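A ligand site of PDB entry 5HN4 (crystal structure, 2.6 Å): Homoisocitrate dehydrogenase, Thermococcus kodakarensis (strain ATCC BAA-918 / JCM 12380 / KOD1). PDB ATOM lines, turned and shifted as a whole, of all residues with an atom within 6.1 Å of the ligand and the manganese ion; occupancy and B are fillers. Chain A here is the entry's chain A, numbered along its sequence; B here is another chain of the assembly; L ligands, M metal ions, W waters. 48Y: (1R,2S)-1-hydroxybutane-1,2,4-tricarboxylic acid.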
ATOM      1  N   THR A  69     -19.841  26.893 -27.617  1.00  0.00           N
ATOM      2  CA  THR A  69     -19.984  27.747 -28.785  1.00  0.00           C
ATOM      3  C   THR A  69     -20.880  28.900 -28.448  1.00  0.00           C
ATOM      4  O   THR A  69     -21.886  28.710 -27.782  1.00  0.00           O
ATOM      5  CB  THR A  69     -20.609  26.957 -29.947  1.00  0.00           C
ATOM      6  OG1 THR A  69     -20.697  27.803 -31.080  1.00  0.00           O
ATOM      7  CG2 THR A  69     -22.016  26.372 -29.585  1.00  0.00           C
ATOM      8  N   THR A  71     -23.874  31.015 -29.298  1.00  0.00           N
ATOM      9  CA  THR A  71     -25.031  31.101 -30.178  1.00  0.00           C
ATOM     10  C   THR A  71     -25.684  32.485 -30.011  1.00  0.00           C
ATOM     11  O   THR A  71     -26.424  32.690 -29.045  1.00  0.00           O
ATOM     12  CB  THR A  71     -26.074  29.981 -29.905  1.00  0.00           C
ATOM     13  OG1 THR A  71     -25.509  28.697 -30.246  1.00  0.00           O
ATOM     14  CG2 THR A  71     -27.358  30.185 -30.732  1.00  0.00           C
ATOM     15  N   SER A  80     -27.743  26.675 -33.785  1.00  0.00           N
ATOM     16  CA  SER A  80     -26.776  26.142 -32.841  1.00  0.00           C
ATOM     17  C   SER A  80     -25.863  25.029 -33.404  1.00  0.00           C
ATOM     18  O   SER A  80     -26.325  24.029 -33.973  1.00  0.00           O
ATOM     19  CB  SER A  80     -27.506  25.552 -31.613  1.00  0.00           C
ATOM     20  OG  SER A  80     -26.778  25.751 -30.417  1.00  0.00           O
ATOM     21  N   LEU A  81     -24.555  25.225 -33.259  1.00  0.00           N
ATOM     22  CA  LEU A  81     -23.643  24.117 -33.481  1.00  0.00           C
ATOM     23  C   LEU A  81     -24.058  22.853 -32.729  1.00  0.00           C
ATOM     24  O   LEU A  81     -24.172  21.768 -33.338  1.00  0.00           O
ATOM     25  CB  LEU A  81     -22.248  24.507 -33.058  1.00  0.00           C
ATOM     26  CG  LEU A  81     -21.164  23.477 -33.355  1.00  0.00           C
ATOM     27  CD1 LEU A  81     -21.294  22.915 -34.779  1.00  0.00           C
ATOM     28  CD2 LEU A  81     -19.830  24.162 -33.143  1.00  0.00           C
ATOM     29  N   ILE A  82     -24.293  22.974 -31.421  1.00  0.00           N
ATOM     30  CA  ILE A  82     -24.583  21.774 -30.630  1.00  0.00           C
ATOM     31  C   ILE A  82     -25.932  21.176 -30.966  1.00  0.00           C
ATOM     32  O   ILE A  82     -26.088  19.941 -30.997  1.00  0.00           O
ATOM     33  CB  ILE A  82     -24.418  21.976 -29.092  1.00  0.00           C
ATOM     34  CG1 ILE A  82     -24.495  20.639 -28.352  1.00  0.00           C
ATOM     35  CG2 ILE A  82     -25.439  22.926 -28.484  1.00  0.00           C
ATOM     36  CD1 ILE A  82     -23.260  19.776 -28.528  1.00  0.00           C
ATOM     37  N   LEU A  83     -26.921  22.006 -31.262  1.00  0.00           N
ATOM     38  CA  LEU A  83     -28.233  21.435 -31.684  1.00  0.00           C
ATOM     39  C   LEU A  83     -28.107  20.749 -33.002  1.00  0.00           C
ATOM     40  O   LEU A  83     -28.668  19.662 -33.188  1.00  0.00           O
ATOM     41  CB  LEU A  83     -29.357  22.469 -31.780  1.00  0.00           C
ATOM     42  CG  LEU A  83     -29.646  23.164 -30.441  1.00  0.00           C
ATOM     43  CD1 LEU A  83     -30.741  24.204 -30.623  1.00  0.00           C
ATOM     44  CD2 LEU A  83     -29.973  22.154 -29.331  1.00  0.00           C
ATOM     45  N   ARG A  86     -26.336  17.530 -32.350  1.00  0.00           N
ATOM     46  CA  ARG A  86     -27.248  16.588 -31.714  1.00  0.00           C
ATOM     47  C   ARG A  86     -28.168  15.884 -32.709  1.00  0.00           C
ATOM     48  O   ARG A  86     -28.325  14.661 -32.617  1.00  0.00           O
ATOM     49  CB  ARG A  86     -28.065  17.280 -30.644  1.00  0.00           C
ATOM     50  CG  ARG A  86     -27.282  17.526 -29.365  1.00  0.00           C
ATOM     51  CD  ARG A  86     -28.155  18.273 -28.364  1.00  0.00           C
ATOM     52  NE  ARG A  86     -27.385  18.784 -27.261  1.00  0.00           N
ATOM     53  CZ  ARG A  86     -27.800  19.742 -26.447  1.00  0.00           C
ATOM     54  NH1 ARG A  86     -29.009  20.311 -26.596  1.00  0.00           N
ATOM     55  NH2 ARG A  86     -26.990  20.144 -25.471  1.00  0.00           N
ATOM     56  N   ASN A  94     -29.324  12.720 -23.211  1.00  0.00           N
ATOM     57  CA  ASN A  94     -28.405  13.722 -22.680  1.00  0.00           C
ATOM     58  C   ASN A  94     -28.318  13.514 -21.176  1.00  0.00           C
ATOM     59  O   ASN A  94     -29.277  13.711 -20.461  1.00  0.00           O
ATOM     60  CB  ASN A  94     -28.918  15.103 -23.046  1.00  0.00           C
ATOM     61  CG  ASN A  94     -28.068  16.216 -22.520  1.00  0.00           C
ATOM     62  OD1 ASN A  94     -27.480  16.138 -21.455  1.00  0.00           O
ATOM     63  ND2 ASN A  94     -28.046  17.302 -23.247  1.00  0.00           N
ATOM     64  N   ARG A  96     -26.688  14.417 -17.583  1.00  0.00           N
ATOM     65  CA  ARG A  96     -25.948  15.435 -16.840  1.00  0.00           C
ATOM     66  C   ARG A  96     -25.816  14.993 -15.402  1.00  0.00           C
ATOM     67  O   ARG A  96     -26.777  14.559 -14.792  1.00  0.00           O
ATOM     68  CB  ARG A  96     -26.628  16.785 -16.968  1.00  0.00           C
ATOM     69  CG  ARG A  96     -26.483  17.322 -18.372  1.00  0.00           C
ATOM     70  CD  ARG A  96     -27.443  18.441 -18.773  1.00  0.00           C
ATOM     71  NE  ARG A  96     -27.176  18.855 -20.160  1.00  0.00           N
ATOM     72  CZ  ARG A  96     -27.480  20.036 -20.687  1.00  0.00           C
ATOM     73  NH1 ARG A  96     -28.096  21.003 -19.997  1.00  0.00           N
ATOM     74  NH2 ARG A  96     -27.172  20.244 -21.966  1.00  0.00           N
ATOM     75  N   ARG A 111     -31.979  13.752 -19.767  1.00  0.00           N
ATOM     76  CA  ARG A 111     -32.808  14.690 -20.536  1.00  0.00           C
ATOM     77  C   ARG A 111     -33.021  14.092 -21.896  1.00  0.00           C
ATOM     78  O   ARG A 111     -32.070  13.851 -22.630  1.00  0.00           O
ATOM     79  CB  ARG A 111     -32.094  16.042 -20.650  1.00  0.00           C
ATOM     80  CG  ARG A 111     -32.456  16.910 -21.874  1.00  0.00           C
ATOM     81  CD  ARG A 111     -31.642  18.202 -21.928  1.00  0.00           C
ATOM     82  NE  ARG A 111     -32.054  19.032 -23.049  1.00  0.00           N
ATOM     83  CZ  ARG A 111     -31.530  20.213 -23.375  1.00  0.00           C
ATOM     84  NH1 ARG A 111     -32.008  20.879 -24.409  1.00  0.00           N
ATOM     85  NH2 ARG A 111     -30.537  20.725 -22.670  1.00  0.00           N
ATOM     86  N   ASN A 113     -33.271  14.018 -25.615  1.00  0.00           N
ATOM     87  CA  ASN A 113     -32.406  14.943 -26.345  1.00  0.00           C
ATOM     88  C   ASN A 113     -32.735  15.171 -27.809  1.00  0.00           C
ATOM     89  O   ASN A 113     -32.036  15.936 -28.477  1.00  0.00           O
ATOM     90  CB  ASN A 113     -30.962  14.455 -26.234  1.00  0.00           C
ATOM     91  CG  ASN A 113     -29.939  15.569 -26.336  1.00  0.00           C
ATOM     92  OD1 ASN A 113     -30.178  16.698 -25.892  1.00  0.00           O
ATOM     93  ND2 ASN A 113     -28.774  15.249 -26.866  1.00  0.00           N
ATOM     94  N   TYR A 118     -38.080  20.660 -28.756  1.00  0.00           N
ATOM     95  CA  TYR A 118     -36.925  20.798 -29.649  1.00  0.00           C
ATOM     96  C   TYR A 118     -37.169  20.125 -31.001  1.00  0.00           C
ATOM     97  O   TYR A 118     -36.335  20.237 -31.892  1.00  0.00           O
ATOM     98  CB  TYR A 118     -35.639  20.178 -29.012  1.00  0.00           C
ATOM     99  CG  TYR A 118     -34.989  21.042 -27.962  1.00  0.00           C
ATOM    100  CD1 TYR A 118     -35.553  21.182 -26.688  1.00  0.00           C
ATOM    101  CD2 TYR A 118     -33.820  21.753 -28.248  1.00  0.00           C
ATOM    102  CE1 TYR A 118     -34.973  21.994 -25.745  1.00  0.00           C
ATOM    103  CE2 TYR A 118     -33.228  22.566 -27.313  1.00  0.00           C
ATOM    104  CZ  TYR A 118     -33.802  22.691 -26.072  1.00  0.00           C
ATOM    105  OH  TYR A 118     -33.172  23.478 -25.145  1.00  0.00           O
ATOM    106  N   ASN A 214     -37.284  17.038 -23.134  1.00  0.00           N
ATOM    107  CA  ASN A 214     -36.123  17.818 -23.521  1.00  0.00           C
ATOM    108  C   ASN A 214     -36.006  19.183 -22.867  1.00  0.00           C
ATOM    109  O   ASN A 214     -35.011  19.460 -22.176  1.00  0.00           O
ATOM    110  CB  ASN A 214     -36.134  17.956 -25.032  1.00  0.00           C
ATOM    111  CG  ASN A 214     -34.787  18.235 -25.617  1.00  0.00           C
ATOM    112  OD1 ASN A 214     -33.962  18.933 -25.039  1.00  0.00           O
ATOM    113  ND2 ASN A 214     -34.568  17.729 -26.800  1.00  0.00           N
ATOM    114  N   ASP A 218     -33.639  20.614 -19.927  1.00  0.00           N
ATOM    115  CA  ASP A 218     -32.786  21.769 -20.085  1.00  0.00           C
ATOM    116  C   ASP A 218     -32.895  22.681 -18.870  1.00  0.00           C
ATOM    117  O   ASP A 218     -31.885  23.168 -18.345  1.00  0.00           O
ATOM    118  CB  ASP A 218     -33.176  22.505 -21.360  1.00  0.00           C
ATOM    119  CG  ASP A 218     -32.330  23.701 -21.606  1.00  0.00           C
ATOM    120  OD1 ASP A 218     -31.080  23.522 -21.771  1.00  0.00           O
ATOM    121  OD2 ASP A 218     -32.913  24.809 -21.661  1.00  0.00           O
ATOM    122  N   ILE A 219     -34.126  22.930 -18.445  1.00  0.00           N
ATOM    123  CA  ILE A 219     -34.401  23.788 -17.321  1.00  0.00           C
ATOM    124  C   ILE A 219     -33.912  23.161 -16.017  1.00  0.00           C
ATOM    125  O   ILE A 219     -33.228  23.807 -15.254  1.00  0.00           O
ATOM    126  CB  ILE A 219     -35.890  24.099 -17.214  1.00  0.00           C
ATOM    127  CG1 ILE A 219     -36.317  24.950 -18.413  1.00  0.00           C
ATOM    128  CG2 ILE A 219     -36.200  24.820 -15.892  1.00  0.00           C
ATOM    129  CD1 ILE A 219     -37.813  25.112 -18.556  1.00  0.00           C
ATOM    130  N   SER A 221     -31.715  20.812 -15.417  1.00  0.00           N
ATOM    131  CA  SER A 221     -30.297  20.543 -15.306  1.00  0.00           C
ATOM    132  C   SER A 221     -29.500  21.817 -15.021  1.00  0.00           C
ATOM    133  O   SER A 221     -28.553  21.771 -14.249  1.00  0.00           O
ATOM    134  CB  SER A 221     -29.789  19.858 -16.569  1.00  0.00           C
ATOM    135  OG  SER A 221     -29.933  20.707 -17.685  1.00  0.00           O
ATOM    136  N   ASP A 222     -29.861  22.952 -15.622  1.00  0.00           N
ATOM    137  CA  ASP A 222     -29.263  24.206 -15.149  1.00  0.00           C
ATOM    138  C   ASP A 222     -29.601  24.469 -13.691  1.00  0.00           C
ATOM    139  O   ASP A 222     -28.704  24.781 -12.924  1.00  0.00           O
ATOM    140  CB  ASP A 222     -29.695  25.389 -15.967  1.00  0.00           C
ATOM    141  CG  ASP A 222     -28.716  25.726 -17.053  1.00  0.00           C
ATOM    142  OD1 ASP A 222     -28.113  24.818 -17.646  1.00  0.00           O
ATOM    143  OD2 ASP A 222     -28.574  26.927 -17.323  1.00  0.00           O
ATOM    144  N   GLU A 247     -19.541  17.274 -23.486  1.00  0.00           N
ATOM    145  CA  GLU A 247     -19.350  18.679 -23.333  1.00  0.00           C
ATOM    146  C   GLU A 247     -19.625  19.078 -21.930  1.00  0.00           C
ATOM    147  O   GLU A 247     -20.548  18.552 -21.283  1.00  0.00           O
ATOM    148  CB  GLU A 247     -20.301  19.451 -24.257  1.00  0.00           C
ATOM    149  CG  GLU A 247     -21.778  19.036 -24.110  1.00  0.00           C
ATOM    150  CD  GLU A 247     -22.788  19.958 -24.770  1.00  0.00           C
ATOM    151  OE1 GLU A 247     -23.955  19.516 -24.935  1.00  0.00           O
ATOM    152  OE2 GLU A 247     -22.449  21.108 -25.131  1.00  0.00           O
ATOM    153  N   VAL A 249     -21.337  21.406 -19.283  1.00  0.00           N
ATOM    154  CA  VAL A 249     -22.634  22.080 -19.275  1.00  0.00           C
ATOM    155  C   VAL A 249     -22.487  23.614 -19.287  1.00  0.00           C
ATOM    156  O   VAL A 249     -23.378  24.303 -19.714  1.00  0.00           O
ATOM    157  CB  VAL A 249     -23.481  21.602 -18.074  1.00  0.00           C
ATOM    158  CG1 VAL A 249     -24.755  22.417 -17.915  1.00  0.00           C
ATOM    159  CG2 VAL A 249     -23.819  20.141 -18.271  1.00  0.00           C
ATOM    160  N   LYS B 163     -37.112  31.145 -24.306  1.00  0.00           N
ATOM    161  CA  LYS B 163     -36.179  30.266 -24.993  1.00  0.00           C
ATOM    162  C   LYS B 163     -36.360  30.471 -26.490  1.00  0.00           C
ATOM    163  O   LYS B 163     -36.591  29.537 -27.242  1.00  0.00           O
ATOM    164  CB  LYS B 163     -36.474  28.797 -24.630  1.00  0.00           C
ATOM    165  CG  LYS B 163     -35.418  27.778 -25.080  1.00  0.00           C
ATOM    166  CD  LYS B 163     -34.115  27.849 -24.266  1.00  0.00           C
ATOM    167  CE  LYS B 163     -33.287  26.564 -24.405  1.00  0.00           C
ATOM    168  NZ  LYS B 163     -31.994  26.466 -23.645  1.00  0.00           N
ATOM    169  N   ASN B 165     -34.272  30.975 -28.906  1.00  0.00           N
ATOM    170  CA  ASN B 165     -33.480  30.201 -29.853  1.00  0.00           C
ATOM    171  C   ASN B 165     -34.198  28.957 -30.358  1.00  0.00           C
ATOM    172  O   ASN B 165     -33.989  28.556 -31.488  1.00  0.00           O
ATOM    173  CB  ASN B 165     -32.135  29.798 -29.267  1.00  0.00           C
ATOM    174  CG  ASN B 165     -31.202  30.989 -29.097  1.00  0.00           C
ATOM    175  OD1 ASN B 165     -31.527  32.123 -29.461  1.00  0.00           O
ATOM    176  ND2 ASN B 165     -30.038  30.718 -28.544  1.00  0.00           N
ATOM    177  N   VAL B 166     -35.070  28.375 -29.539  1.00  0.00           N
ATOM    178  CA  VAL B 166     -35.688  27.116 -29.841  1.00  0.00           C
ATOM    179  C   VAL B 166     -37.149  27.284 -30.173  1.00  0.00           C
ATOM    180  O   VAL B 166     -37.694  26.477 -30.921  1.00  0.00           O
ATOM    181  CB  VAL B 166     -35.541  26.143 -28.644  1.00  0.00           C
ATOM    182  CG1 VAL B 166     -36.219  24.812 -28.864  1.00  0.00           C
ATOM    183  CG2 VAL B 166     -34.090  25.889 -28.340  1.00  0.00           C
ATOM    184  N   ASP B 194     -33.480  28.514 -18.905  1.00  0.00           N
ATOM    185  CA  ASP B 194     -32.593  27.583 -18.163  1.00  0.00           C
ATOM    186  C   ASP B 194     -31.662  28.322 -17.240  1.00  0.00           C
ATOM    187  O   ASP B 194     -31.692  28.108 -16.024  1.00  0.00           O
ATOM    188  CB  ASP B 194     -31.806  26.570 -19.054  1.00  0.00           C
ATOM    189  CG  ASP B 194     -31.093  27.212 -20.249  1.00  0.00           C
ATOM    190  OD1 ASP B 194     -31.266  28.423 -20.476  1.00  0.00           O
ATOM    191  OD2 ASP B 194     -30.402  26.486 -20.986  1.00  0.00           O
ATOM    192  N   SER B 195     -30.854  29.206 -17.795  1.00  0.00           N
ATOM    193  CA  SER B 195     -29.898  29.959 -16.980  1.00  0.00           C
ATOM    194  C   SER B 195     -30.585  30.877 -15.965  1.00  0.00           C
ATOM    195  O   SER B 195     -30.037  31.149 -14.892  1.00  0.00           O
ATOM    196  CB  SER B 195     -28.933  30.770 -17.873  1.00  0.00           C
ATOM    197  OG  SER B 195     -29.636  31.557 -18.797  1.00  0.00           O
HETATM  198  OAB 48Y L   1     -27.143  22.399 -23.775  1.00  0.00           O
HETATM  199  CAK 48Y L   1     -27.776  23.292 -23.178  1.00  0.00           C
HETATM  200  OAF 48Y L   1     -28.328  23.121 -22.077  1.00  0.00           O
HETATM  201  CAM 48Y L   1     -27.884  24.654 -23.906  1.00  0.00           C
HETATM  202  OAD 48Y L   1     -28.785  25.556 -23.243  1.00  0.00           O
HETATM  203  CAN 48Y L   1     -28.357  24.439 -25.325  1.00  0.00           C
HETATM  204  CAL 48Y L   1     -29.797  23.826 -25.280  1.00  0.00           C
HETATM  205  OAG 48Y L   1     -29.929  22.589 -25.067  1.00  0.00           O
HETATM  206  OAC 48Y L   1     -30.734  24.615 -25.457  1.00  0.00           O
HETATM  207  CAI 48Y L   1     -28.265  25.788 -25.969  1.00  0.00           C
HETATM  208  CAH 48Y L   1     -28.655  25.660 -27.446  1.00  0.00           C
HETATM  209  CAJ 48Y L   1     -28.558  27.046 -28.133  1.00  0.00           C
HETATM  210  OAE 48Y L   1     -29.642  27.657 -28.356  1.00  0.00           O
HETATM  211  OAA 48Y L   1     -27.407  27.471 -28.405  1.00  0.00           O
HETATM  212 MN    MN M   1     -29.501  24.707 -21.291  1.00  0.00          MN
HETATM  213  O   HOH W   1     -29.383  23.513 -19.435  1.00  0.00           O
HETATM  214  O   HOH W   2     -27.515  25.517 -20.290  1.00  0.00           O
HETATM  215  O   HOH W   3     -31.097  28.855 -25.797  1.00  0.00           O
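The side-chain hydroxyl of Tyr 118 lies within hydrogen-bond range of an oxygen (OAC) of the ligand (2.7 Å). An oxygen (OAA) of the ligand lies within hydrogen-bond range of the side-chain hydroxyl (OG) of Ser 80 (2.7 Å). OAC of the ligand is in salt-bridge range of NZ of Lys 163 of chain B, 2.9 Å away. The side-chain amide nitrogen of Asn 165 of chain B sits at hydrogen-bond distance from an oxygen (OAE) of the ligand (3.1 Å). The guanidinium group of Arg 111 lies within salt-bridge range of an oxygen (OAG) of the ligand (2.8 Å). NH2 of Arg 96 lies within salt-bridge range of OAB of the ligand, 2.8 Å away. OAA of the ligand lies within hydrogen-bond range of OG1 of Thr 71, at 2.9 Å. NH2 of Arg 86 is in salt-bridge range of OAB of the ligand.
The side-chain amide oxygen of Asn 214 is in hydrogen-bond range of the guanidinium group of Arg 111 (2.8 Å). OE1 of Glu 247 lies within salt-bridge range of NH2 of Arg 86. The side-chain carboxylate (OD2) of Asp 222 sits at hydrogen-bond distance from the backbone NH (N) of Ser 195 of chain B. OH of Tyr 118 lies within hydrogen-bond range of NH1 of Arg 111, at 2.9 Å. The backbone carbonyl oxygen (O) of Asn 94 is in hydrogen-bond range of the backbone NH (N) of Arg 111, at 2.8 Å. The side-chain carboxylate (OD2) of Asp 218 lies within salt-bridge range of the side-chain amino group (NZ) of Lys 163 of chain B, at 2.7 Å. NE of Arg 96 sits at hydrogen-bond distance from OD1 of Asn 94, 3.0 Å away. OD1 of Asp 218 sits close to NH2 of Arg 111, 3.0 Å away.
Hydrophobic or aromatic side chains within 4 Å of the ligand: Tyr 118. Ten residues have an atom within 4 Å of the ligand: Thr 71, Ser 80, Arg 86, Arg 96, Arg 111, Tyr 118, Asp 218, Lys 163 of chain B, Asn 165 of chain B and Asp 194 of chain B.
Residues that only touch the manganese ion: Lys 163 of chain B and Asp 222. The nearest printed residue that does not touch the manganese ion is Arg 96 (4.2 Å).
The manganese ion is bound by OD2 of Asp 194 of chain B, 2.0 Å away. OD1 of Asp 218 is bound to the manganese ion, 2.0 Å away. The manganese ion is bound by OAF of the ligand. Water W1 binds the manganese ion (2.2 Å). OAD of the ligand binds the manganese ion, at 2.2 Å. Water W2 binds the manganese ion (2.4 Å).
Water W1 lies within hydrogen-bond range of OD1 of Asp 222 (2.6 Å), O of Asp 218 (2.8 Å), NH1 of Arg 96 (2.9 Å) and OG of Ser 221 (3.4 Å). Water W3 lies within hydrogen-bond range of OAE of the ligand, NZ of Lys 163 of chain B and ND2 of Asn 165 of chain B.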
